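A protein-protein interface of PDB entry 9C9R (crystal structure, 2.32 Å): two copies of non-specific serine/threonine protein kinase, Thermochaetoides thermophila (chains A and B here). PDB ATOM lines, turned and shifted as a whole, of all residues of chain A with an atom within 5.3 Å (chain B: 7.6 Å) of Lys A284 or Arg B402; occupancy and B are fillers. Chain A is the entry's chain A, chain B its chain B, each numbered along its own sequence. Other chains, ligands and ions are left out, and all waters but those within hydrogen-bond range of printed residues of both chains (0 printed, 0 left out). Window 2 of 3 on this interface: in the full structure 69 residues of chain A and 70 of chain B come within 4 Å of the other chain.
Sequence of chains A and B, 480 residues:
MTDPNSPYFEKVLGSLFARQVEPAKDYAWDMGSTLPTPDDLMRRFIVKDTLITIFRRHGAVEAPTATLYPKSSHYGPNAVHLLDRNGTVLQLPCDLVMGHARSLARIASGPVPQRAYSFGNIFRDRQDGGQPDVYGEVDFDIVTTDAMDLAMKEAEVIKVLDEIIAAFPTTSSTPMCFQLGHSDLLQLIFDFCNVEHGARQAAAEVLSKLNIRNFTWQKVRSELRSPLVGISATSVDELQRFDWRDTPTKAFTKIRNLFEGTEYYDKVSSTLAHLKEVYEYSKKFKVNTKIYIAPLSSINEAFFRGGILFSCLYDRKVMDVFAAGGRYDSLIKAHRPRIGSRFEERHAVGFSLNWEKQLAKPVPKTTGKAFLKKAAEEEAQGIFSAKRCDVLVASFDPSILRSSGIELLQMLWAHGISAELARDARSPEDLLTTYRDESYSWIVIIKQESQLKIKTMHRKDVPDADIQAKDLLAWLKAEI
No position is printed for both chains.
Of the 14 pairs that touch across the chains among the printed residues, none has its exchanged pair printed and touching as well.
Among the printed residues, merely in contact across the chains: Phe A285 with Ile B406, Phe A285 with Gln B410, Met A148 with Asp B424, Tyr A281 with Arg B402, Lys A284 with Ile B406, Met A148 with Arg B402, Lys A286 with Gln B410, Met A152 with Leu B421, Lys A286 with Glu B407, Lys A284 with Gln B410 and Met A152 with Arg B402.
Of chain B, only Arg B402 (3.2 Å), Ile B406 (3.6 Å), Glu B407 (2.9 Å) and Gln B410 (3.7 Å) come within 4 Å of Lys A284.
Arg B402 touches just these residues of chain A: Met A148, Asp A149, Met A152, Tyr A281 and Lys A284.
Of the printed residues of chain A, Gln B410 touches Lys A284 (3.7 Å), Phe A285 (3.5 Å) and Lys A286 (3.7 Å).
Printed residues of chain A within 4 Å of Ile B406: Lys A284 (3.6 Å) and Phe A285 (3.4 Å).
Of the printed residues of chain A, Leu B421 touches Met A152.
Of the printed residues of chain B, Met A148 touches Arg B402 and Asp B424.
Of the printed residues of chain B, Asp A149 touches Arg B402 (3.0 Å).
Ala B422 touches none of the printed residues of chain A.
The nearest residue of chain B that does not touch Lys A284 is Ser B403 (4.1 Å).
The nearest printed residue of chain A that does not touch Arg B402 is Glu A280 (7.3 Å).
OD2 of Asp A149 is in salt-bridge range of NH2 of Arg B402, at 3.0 Å.
The backbone carbonyl oxygen (O) of Lys A284 sits close to the side-chain carboxylate (OE2) of Glu B407, 2.9 Å away.
The side-chain amino group of Lys A284 sits at hydrogen-bond distance from the backbone carbonyl oxygen of Arg B402 (3.2 Å).
Of the 22 printed residues of chain B, 6 touch a printed residue of chain A.
Hydrophobic or aromatic side chains of chain B within 4 Å of the printed part of chain A: Ile B406 and Leu B421.
Along chain B the printed residues that touch a printed residue of chain A span positions 402 to 424.
Printed residues of chain A that touch a printed residue of chain B: Met A148, Asp A149, Met A152, Tyr A281, Lys A284, Phe A285 and Lys A286.
Among the printed residues, Asp or Glu carboxylates within 4 Å of a Lys or Arg side-chain nitrogen of the other chain: Asp A149 with Arg B402.
The backbone carbonyl oxygen of Glu B407 is in hydrogen-bond range of the side-chain amide nitrogen of Gln B410, at 2.9 Å.
The guanidinium group (NH2) of Arg B402 lies within salt-bridge range of the side-chain carboxylate (OD2) of Asp B424, at 2.7 Å.
O of Pro B398 sits at hydrogen-bond distance from NH1 of Arg B402 (2.9 Å).
OD1 of Asp A149 lies within hydrogen-bond range of OH of Tyr A281, at 3.4 Å.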
ATOM      1  N   MET A 148      -3.907  21.732  -1.689  1.00  0.00           N
ATOM      2  CA  MET A 148      -2.502  21.418  -1.932  1.00  0.00           C
ATOM      3  C   MET A 148      -2.141  21.715  -3.385  1.00  0.00           C
ATOM      4  O   MET A 148      -2.840  21.287  -4.311  1.00  0.00           O
ATOM      5  CB  MET A 148      -2.207  19.943  -1.613  1.00  0.00           C
ATOM      6  CG  MET A 148      -1.972  19.597  -0.135  1.00  0.00           C
ATOM      7  SD  MET A 148      -0.279  19.864   0.484  1.00  0.00           S
ATOM      8  CE  MET A 148       0.612  18.468  -0.217  1.00  0.00           C
ATOM      9  N   ASP A 149      -1.055  22.468  -3.579  1.00  0.00           N
ATOM     10  CA  ASP A 149      -0.407  22.627  -4.889  1.00  0.00           C
ATOM     11  C   ASP A 149      -1.366  23.159  -5.958  1.00  0.00           C
ATOM     12  O   ASP A 149      -1.388  22.684  -7.096  1.00  0.00           O
ATOM     13  CB  ASP A 149       0.238  21.306  -5.329  1.00  0.00           C
ATOM     14  CG  ASP A 149       1.428  20.910  -4.441  1.00  0.00           C
ATOM     15  OD1 ASP A 149       2.515  21.513  -4.596  1.00  0.00           O
ATOM     16  OD2 ASP A 149       1.265  20.023  -3.569  1.00  0.00           O
ATOM     17  N   MET A 152       0.606  24.241  -9.013  1.00  0.00           N
ATOM     18  CA  MET A 152       1.065  23.151  -9.885  1.00  0.00           C
ATOM     19  C   MET A 152      -0.022  22.737 -10.876  1.00  0.00           C
ATOM     20  O   MET A 152       0.219  22.658 -12.091  1.00  0.00           O
ATOM     21  CB  MET A 152       1.495  21.951  -9.044  1.00  0.00           C
ATOM     22  CG  MET A 152       2.338  20.932  -9.792  1.00  0.00           C
ATOM     23  SD  MET A 152       2.156  19.327  -8.972  1.00  0.00           S
ATOM     24  CE  MET A 152       2.934  19.672  -7.385  1.00  0.00           C
ATOM     25  N   GLU A 280       7.300  29.165 -12.016  1.00  0.00           N
ATOM     26  CA  GLU A 280       8.336  28.162 -11.778  1.00  0.00           C
ATOM     27  C   GLU A 280       7.917  26.813 -12.333  1.00  0.00           C
ATOM     28  O   GLU A 280       8.662  26.183 -13.089  1.00  0.00           O
ATOM     29  CB  GLU A 280       8.648  28.025 -10.289  1.00  0.00           C
ATOM     30  CG  GLU A 280       8.900  29.334  -9.531  1.00  0.00           C
ATOM     31  CD  GLU A 280      10.152  30.104  -9.974  1.00  0.00           C
ATOM     32  OE1 GLU A 280      10.545  31.055  -9.261  1.00  0.00           O
ATOM     33  OE2 GLU A 280      10.763  29.759 -11.018  1.00  0.00           O
ATOM     34  N   TYR A 281       6.711  26.363 -11.979  1.00  0.00           N
ATOM     35  CA  TYR A 281       6.254  25.069 -12.447  1.00  0.00           C
ATOM     36  C   TYR A 281       6.159  25.029 -13.964  1.00  0.00           C
ATOM     37  O   TYR A 281       6.432  23.990 -14.572  1.00  0.00           O
ATOM     38  CB  TYR A 281       4.912  24.732 -11.815  1.00  0.00           C
ATOM     39  CG  TYR A 281       4.983  24.187 -10.408  1.00  0.00           C
ATOM     40  CD1 TYR A 281       5.702  23.032 -10.121  1.00  0.00           C
ATOM     41  CD2 TYR A 281       4.304  24.805  -9.370  1.00  0.00           C
ATOM     42  CE1 TYR A 281       5.753  22.525  -8.828  1.00  0.00           C
ATOM     43  CE2 TYR A 281       4.357  24.300  -8.079  1.00  0.00           C
ATOM     44  CZ  TYR A 281       5.076  23.160  -7.819  1.00  0.00           C
ATOM     45  OH  TYR A 281       5.116  22.659  -6.540  1.00  0.00           O
ATOM     46  N   SER A 282       5.820  26.147 -14.607  1.00  0.00           N
ATOM     47  CA  SER A 282       5.705  26.071 -16.060  1.00  0.00           C
ATOM     48  C   SER A 282       7.068  25.863 -16.715  1.00  0.00           C
ATOM     49  O   SER A 282       7.153  25.247 -17.786  1.00  0.00           O
ATOM     50  CB  SER A 282       5.000  27.314 -16.617  1.00  0.00           C
ATOM     51  OG  SER A 282       5.871  28.433 -16.675  1.00  0.00           O
ATOM     52  N   LYS A 283       8.141  26.348 -16.079  1.00  0.00           N
ATOM     53  CA  LYS A 283       9.489  26.048 -16.552  1.00  0.00           C
ATOM     54  C   LYS A 283       9.840  24.579 -16.323  1.00  0.00           C
ATOM     55  O   LYS A 283      10.431  23.935 -17.195  1.00  0.00           O
ATOM     56  CB  LYS A 283      10.507  26.969 -15.866  1.00  0.00           C
ATOM     57  CG  LYS A 283      10.561  28.382 -16.468  1.00  0.00           C
ATOM     58  CD  LYS A 283      11.650  29.259 -15.843  1.00  0.00           C
ATOM     59  CE  LYS A 283      11.360  29.578 -14.380  1.00  0.00           C
ATOM     60  NZ  LYS A 283      12.244  30.665 -13.834  1.00  0.00           N
ATOM     61  N   LYS A 284       9.476  24.029 -15.161  1.00  0.00           N
ATOM     62  CA  LYS A 284       9.699  22.607 -14.920  1.00  0.00           C
ATOM     63  C   LYS A 284       8.910  21.730 -15.905  1.00  0.00           C
ATOM     64  O   LYS A 284       9.416  20.702 -16.371  1.00  0.00           O
ATOM     65  CB  LYS A 284       9.337  22.268 -13.475  1.00  0.00           C
ATOM     66  CG  LYS A 284      10.320  22.757 -12.434  1.00  0.00           C
ATOM     67  CD  LYS A 284       9.751  22.544 -11.035  1.00  0.00           C
ATOM     68  CE  LYS A 284      10.661  23.120  -9.964  1.00  0.00           C
ATOM     69  NZ  LYS A 284       9.915  23.449  -8.698  1.00  0.00           N
ATOM     70  N   PHE A 285       7.664  22.104 -16.224  1.00  0.00           N
ATOM     71  CA  PHE A 285       6.942  21.400 -17.280  1.00  0.00           C
ATOM     72  C   PHE A 285       7.529  21.691 -18.670  1.00  0.00           C
ATOM     73  O   PHE A 285       7.069  21.116 -19.669  1.00  0.00           O
ATOM     74  CB  PHE A 285       5.448  21.773 -17.256  1.00  0.00           C
ATOM     75  CG  PHE A 285       4.658  21.161 -16.119  1.00  0.00           C
ATOM     76  CD1 PHE A 285       4.527  19.787 -15.991  1.00  0.00           C
ATOM     77  CD2 PHE A 285       3.983  21.967 -15.214  1.00  0.00           C
ATOM     78  CE1 PHE A 285       3.762  19.227 -14.953  1.00  0.00           C
ATOM     79  CE2 PHE A 285       3.228  21.407 -14.163  1.00  0.00           C
ATOM     80  CZ  PHE A 285       3.112  20.044 -14.037  1.00  0.00           C
ATOM     81  N   LYS A 286       8.521  22.571 -18.758  1.00  0.00           N
ATOM     82  CA  LYS A 286       9.100  23.008 -20.026  1.00  0.00           C
ATOM     83  C   LYS A 286       8.021  23.532 -20.975  1.00  0.00           C
ATOM     84  O   LYS A 286       7.848  23.066 -22.097  1.00  0.00           O
ATOM     85  CB  LYS A 286       9.919  21.884 -20.668  1.00  0.00           C
ATOM     86  CG  LYS A 286      11.077  21.422 -19.792  1.00  0.00           C
ATOM     87  CD  LYS A 286      12.149  20.687 -20.593  1.00  0.00           C
ATOM     88  CE  LYS A 286      13.439  20.582 -19.777  1.00  0.00           C
ATOM     89  NZ  LYS A 286      14.061  21.925 -19.568  1.00  0.00           N
ATOM     90  N   SER B 395       7.710   9.900  -5.405  1.00  0.00           N
ATOM     91  CA  SER B 395       8.962  10.125  -4.686  1.00  0.00           C
ATOM     92  C   SER B 395       8.666  10.390  -3.222  1.00  0.00           C
ATOM     93  O   SER B 395       7.711  11.103  -2.902  1.00  0.00           O
ATOM     94  CB  SER B 395       9.756  11.304  -5.252  1.00  0.00           C
ATOM     95  OG  SER B 395      10.740  11.688  -4.315  1.00  0.00           O
ATOM     96  N   ASP B 397      10.560  12.029  -1.179  1.00  0.00           N
ATOM     97  CA  ASP B 397      11.004  13.343  -0.772  1.00  0.00           C
ATOM     98  C   ASP B 397      10.087  14.385  -1.387  1.00  0.00           C
ATOM     99  O   ASP B 397      10.063  14.517  -2.623  1.00  0.00           O
ATOM    100  CB  ASP B 397      12.445  13.592  -1.198  1.00  0.00           C
ATOM    101  CG  ASP B 397      13.011  14.860  -0.571  1.00  0.00           C
ATOM    102  OD1 ASP B 397      13.131  14.894   0.678  1.00  0.00           O
ATOM    103  OD2 ASP B 397      13.302  15.823  -1.321  1.00  0.00           O
ATOM    104  N   PRO B 398       9.329  15.142  -0.583  1.00  0.00           N
ATOM    105  CA  PRO B 398       8.416  16.147  -1.159  1.00  0.00           C
ATOM    106  C   PRO B 398       9.088  17.042  -2.183  1.00  0.00           C
ATOM    107  O   PRO B 398       8.517  17.327  -3.241  1.00  0.00           O
ATOM    108  CB  PRO B 398       7.960  16.944   0.067  1.00  0.00           C
ATOM    109  CG  PRO B 398       8.218  16.048   1.238  1.00  0.00           C
ATOM    110  CD  PRO B 398       9.401  15.218   0.885  1.00  0.00           C
ATOM    111  N   SER B 399      10.322  17.452  -1.918  1.00  0.00           N
ATOM    112  CA  SER B 399      10.972  18.406  -2.800  1.00  0.00           C
ATOM    113  C   SER B 399      11.461  17.759  -4.091  1.00  0.00           C
ATOM    114  O   SER B 399      11.574  18.440  -5.114  1.00  0.00           O
ATOM    115  CB  SER B 399      12.121  19.088  -2.048  1.00  0.00           C
ATOM    116  OG  SER B 399      12.968  19.787  -2.940  1.00  0.00           O
ATOM    117  N   ILE B 400      11.766  16.461  -4.079  1.00  0.00           N
ATOM    118  CA  ILE B 400      12.154  15.798  -5.324  1.00  0.00           C
ATOM    119  C   ILE B 400      10.931  15.583  -6.212  1.00  0.00           C
ATOM    120  O   ILE B 400      10.978  15.813  -7.429  1.00  0.00           O
ATOM    121  CB  ILE B 400      12.881  14.472  -5.024  1.00  0.00           C
ATOM    122  CG1 ILE B 400      14.117  14.715  -4.151  1.00  0.00           C
ATOM    123  CG2 ILE B 400      13.279  13.773  -6.314  1.00  0.00           C
ATOM    124  CD1 ILE B 400      15.004  13.480  -4.010  1.00  0.00           C
ATOM    125  N   LEU B 401       9.828  15.131  -5.613  1.00  0.00           N
ATOM    126  CA  LEU B 401       8.547  15.017  -6.299  1.00  0.00           C
ATOM    127  C   LEU B 401       8.228  16.240  -7.140  1.00  0.00           C
ATOM    128  O   LEU B 401       7.783  16.116  -8.286  1.00  0.00           O
ATOM    129  CB  LEU B 401       7.435  14.809  -5.273  1.00  0.00           C
ATOM    130  CG  LEU B 401       6.072  14.482  -5.887  1.00  0.00           C
ATOM    131  CD1 LEU B 401       6.079  13.052  -6.435  1.00  0.00           C
ATOM    132  CD2 LEU B 401       4.958  14.687  -4.866  1.00  0.00           C
ATOM    133  N   ARG B 402       8.459  17.433  -6.584  1.00  0.00           N
ATOM    134  CA  ARG B 402       8.033  18.685  -7.198  1.00  0.00           C
ATOM    135  C   ARG B 402       9.102  19.320  -8.061  1.00  0.00           C
ATOM    136  O   ARG B 402       8.884  20.421  -8.584  1.00  0.00           O
ATOM    137  CB  ARG B 402       7.581  19.679  -6.129  1.00  0.00           C
ATOM    138  CG  ARG B 402       6.204  19.388  -5.598  1.00  0.00           C
ATOM    139  CD  ARG B 402       5.979  20.056  -4.268  1.00  0.00           C
ATOM    140  NE  ARG B 402       4.731  19.596  -3.677  1.00  0.00           N
ATOM    141  CZ  ARG B 402       4.599  18.460  -3.006  1.00  0.00           C
ATOM    142  NH1 ARG B 402       5.633  17.663  -2.787  1.00  0.00           N
ATOM    143  NH2 ARG B 402       3.397  18.107  -2.563  1.00  0.00           N
ATOM    144  N   SER B 403      10.237  18.656  -8.236  1.00  0.00           N
ATOM    145  CA  SER B 403      11.269  19.142  -9.145  1.00  0.00           C
ATOM    146  C   SER B 403      11.524  18.130 -10.260  1.00  0.00           C
ATOM    147  O   SER B 403      10.957  18.252 -11.357  1.00  0.00           O
ATOM    148  CB  SER B 403      12.561  19.434  -8.377  1.00  0.00           C
ATOM    149  OG  SER B 403      12.819  18.397  -7.441  1.00  0.00           O
ATOM    150  N   SER B 404      12.365  17.122  -9.988  1.00  0.00           N
ATOM    151  CA  SER B 404      12.666  16.123 -11.007  1.00  0.00           C
ATOM    152  C   SER B 404      11.446  15.280 -11.356  1.00  0.00           C
ATOM    153  O   SER B 404      11.334  14.806 -12.487  1.00  0.00           O
ATOM    154  CB  SER B 404      13.799  15.222 -10.536  1.00  0.00           C
ATOM    155  OG  SER B 404      13.383  14.493  -9.396  1.00  0.00           O
ATOM    156  N   GLY B 405      10.538  15.068 -10.402  1.00  0.00           N
ATOM    157  CA  GLY B 405       9.244  14.490 -10.695  1.00  0.00           C
ATOM    158  C   GLY B 405       8.577  15.164 -11.878  1.00  0.00           C
ATOM    159  O   GLY B 405       8.239  14.508 -12.867  1.00  0.00           O
ATOM    160  N   ILE B 406       8.402  16.486 -11.796  1.00  0.00           N
ATOM    161  CA  ILE B 406       7.789  17.231 -12.894  1.00  0.00           C
ATOM    162  C   ILE B 406       8.623  17.101 -14.160  1.00  0.00           C
ATOM    163  O   ILE B 406       8.085  17.050 -15.275  1.00  0.00           O
ATOM    164  CB  ILE B 406       7.608  18.710 -12.500  1.00  0.00           C
ATOM    165  CG1 ILE B 406       6.809  18.850 -11.198  1.00  0.00           C
ATOM    166  CG2 ILE B 406       6.996  19.483 -13.634  1.00  0.00           C
ATOM    167  CD1 ILE B 406       5.393  18.312 -11.259  1.00  0.00           C
ATOM    168  N   GLU B 407       9.948  17.044 -14.013  1.00  0.00           N
ATOM    169  CA  GLU B 407      10.816  16.991 -15.188  1.00  0.00           C
ATOM    170  C   GLU B 407      10.679  15.661 -15.908  1.00  0.00           C
ATOM    171  O   GLU B 407      10.631  15.611 -17.144  1.00  0.00           O
ATOM    172  CB  GLU B 407      12.272  17.219 -14.785  1.00  0.00           C
ATOM    173  CG  GLU B 407      13.004  18.220 -15.670  1.00  0.00           C
ATOM    174  CD  GLU B 407      12.691  19.683 -15.304  1.00  0.00           C
ATOM    175  OE1 GLU B 407      12.794  20.035 -14.095  1.00  0.00           O
ATOM    176  OE2 GLU B 407      12.337  20.469 -16.227  1.00  0.00           O
ATOM    177  N   LEU B 408      10.639  14.571 -15.149  1.00  0.00           N
ATOM    178  CA  LEU B 408      10.425  13.269 -15.760  1.00  0.00           C
ATOM    179  C   LEU B 408       9.063  13.217 -16.441  1.00  0.00           C
ATOM    180  O   LEU B 408       8.925  12.674 -17.547  1.00  0.00           O
ATOM    181  CB  LEU B 408      10.543  12.188 -14.692  1.00  0.00           C
ATOM    182  CG  LEU B 408      11.097  10.852 -15.156  1.00  0.00           C
ATOM    183  CD1 LEU B 408      12.525  11.008 -15.681  1.00  0.00           C
ATOM    184  CD2 LEU B 408      11.043   9.906 -13.980  1.00  0.00           C
ATOM    185  N   LEU B 409       8.059  13.819 -15.798  1.00  0.00           N
ATOM    186  CA  LEU B 409       6.693  13.816 -16.306  1.00  0.00           C
ATOM    187  C   LEU B 409       6.618  14.378 -17.725  1.00  0.00           C
ATOM    188  O   LEU B 409       6.062  13.743 -18.628  1.00  0.00           O
ATOM    189  CB  LEU B 409       5.813  14.614 -15.347  1.00  0.00           C
ATOM    190  CG  LEU B 409       4.372  14.197 -15.111  1.00  0.00           C
ATOM    191  CD1 LEU B 409       4.219  12.693 -15.133  1.00  0.00           C
ATOM    192  CD2 LEU B 409       3.912  14.754 -13.762  1.00  0.00           C
ATOM    193  N   GLN B 410       7.172  15.571 -17.951  1.00  0.00           N
ATOM    194  CA  GLN B 410       7.049  16.161 -19.279  1.00  0.00           C
ATOM    195  C   GLN B 410       7.882  15.401 -20.288  1.00  0.00           C
ATOM    196  O   GLN B 410       7.558  15.398 -21.483  1.00  0.00           O
ATOM    197  CB  GLN B 410       7.431  17.648 -19.267  1.00  0.00           C
ATOM    198  CG  GLN B 410       8.851  17.978 -18.840  1.00  0.00           C
ATOM    199  CD  GLN B 410       9.887  17.739 -19.944  1.00  0.00           C
ATOM    200  OE1 GLN B 410       9.652  18.037 -21.124  1.00  0.00           O
ATOM    201  NE2 GLN B 410      11.037  17.190 -19.559  1.00  0.00           N
ATOM    202  N   MET B 411       8.959  14.760 -19.829  1.00  0.00           N
ATOM    203  CA  MET B 411       9.728  13.879 -20.702  1.00  0.00           C
ATOM    204  C   MET B 411       8.835  12.776 -21.265  1.00  0.00           C
ATOM    205  O   MET B 411       8.752  12.575 -22.482  1.00  0.00           O
ATOM    206  CB  MET B 411      10.905  13.297 -19.915  1.00  0.00           C
ATOM    207  CG  MET B 411      11.974  12.618 -20.753  1.00  0.00           C
ATOM    208  SD  MET B 411      11.488  10.962 -21.275  1.00  0.00           S
ATOM    209  CE  MET B 411      11.354  10.125 -19.687  1.00  0.00           C
ATOM    210  N   LEU B 421       1.507  12.614 -11.768  1.00  0.00           N
ATOM    211  CA  LEU B 421       2.300  12.763 -10.557  1.00  0.00           C
ATOM    212  C   LEU B 421       1.546  12.236  -9.339  1.00  0.00           C
ATOM    213  O   LEU B 421       0.327  12.366  -9.231  1.00  0.00           O
ATOM    214  CB  LEU B 421       2.703  14.226 -10.355  1.00  0.00           C
ATOM    215  CG  LEU B 421       3.815  14.543  -9.328  1.00  0.00           C
ATOM    216  CD1 LEU B 421       5.217  14.220  -9.855  1.00  0.00           C
ATOM    217  CD2 LEU B 421       3.754  15.997  -8.854  1.00  0.00           C
ATOM    218  N   ALA B 422       2.279  11.608  -8.436  1.00  0.00           N
ATOM    219  CA  ALA B 422       1.688  11.064  -7.231  1.00  0.00           C
ATOM    220  C   ALA B 422       1.583  12.139  -6.155  1.00  0.00           C
ATOM    221  O   ALA B 422       2.329  13.122  -6.145  1.00  0.00           O
ATOM    222  CB  ALA B 422       2.527   9.890  -6.714  1.00  0.00           C
ATOM    223  N   ARG B 423       0.644  11.940  -5.238  1.00  0.00           N
ATOM    224  CA  ARG B 423       0.629  12.727  -4.017  1.00  0.00           C
ATOM    225  C   ARG B 423       1.833  12.360  -3.153  1.00  0.00           C
ATOM    226  O   ARG B 423       2.521  11.366  -3.395  1.00  0.00           O
ATOM    227  CB  ARG B 423      -0.672  12.496  -3.254  1.00  0.00           C
ATOM    228  CG  ARG B 423      -1.878  13.114  -3.929  1.00  0.00           C
ATOM    229  CD  ARG B 423      -3.181  12.702  -3.266  1.00  0.00           C
ATOM    230  NE  ARG B 423      -3.280  13.113  -1.870  1.00  0.00           N
ATOM    231  CZ  ARG B 423      -3.704  14.304  -1.463  1.00  0.00           C
ATOM    232  NH1 ARG B 423      -4.007  15.263  -2.324  1.00  0.00           N
ATOM    233  NH2 ARG B 423      -3.828  14.538  -0.158  1.00  0.00           N
ATOM    234  N   ASP B 424       2.097  13.181  -2.140  1.00  0.00           N
ATOM    235  CA  ASP B 424       3.181  12.888  -1.210  1.00  0.00           C
ATOM    236  C   ASP B 424       2.947  11.547  -0.525  1.00  0.00           C
ATOM    237  O   ASP B 424       1.808  11.129  -0.309  1.00  0.00           O
ATOM    238  CB  ASP B 424       3.310  13.993  -0.152  1.00  0.00           C
ATOM    239  CG  ASP B 424       3.960  15.250  -0.692  1.00  0.00           C
ATOM    240  OD1 ASP B 424       5.006  15.141  -1.370  1.00  0.00           O
ATOM    241  OD2 ASP B 424       3.411  16.348  -0.450  1.00  0.00           O
ATOM    242  N   ALA B 425       4.048  10.868  -0.189  1.00  0.00           N
ATOM    243  CA  ALA B 425       3.997   9.584   0.499  1.00  0.00           C
ATOM    244  C   ALA B 425       5.291   9.379   1.276  1.00  0.00           C
ATOM    245  O   ALA B 425       6.372   9.744   0.803  1.00  0.00           O
ATOM    246  CB  ALA B 425       3.776   8.431  -0.487  1.00  0.00           C
ATOM    247  N   ILE B 446      11.303   8.119  -7.628  1.00  0.00           N
ATOM    248  CA  ILE B 446      12.550   8.858  -7.782  1.00  0.00           C
ATOM    249  C   ILE B 446      13.247   8.928  -6.435  1.00  0.00           C
ATOM    250  O   ILE B 446      12.627   9.266  -5.417  1.00  0.00           O
ATOM    251  CB  ILE B 446      12.293  10.263  -8.342  1.00  0.00           C
ATOM    252  CG1 ILE B 446      11.205  10.210  -9.420  1.00  0.00           C
ATOM    253  CG2 ILE B 446      13.573  10.844  -8.899  1.00  0.00           C
ATOM    254  CD1 ILE B 446      11.008  11.509 -10.149  1.00  0.00           C
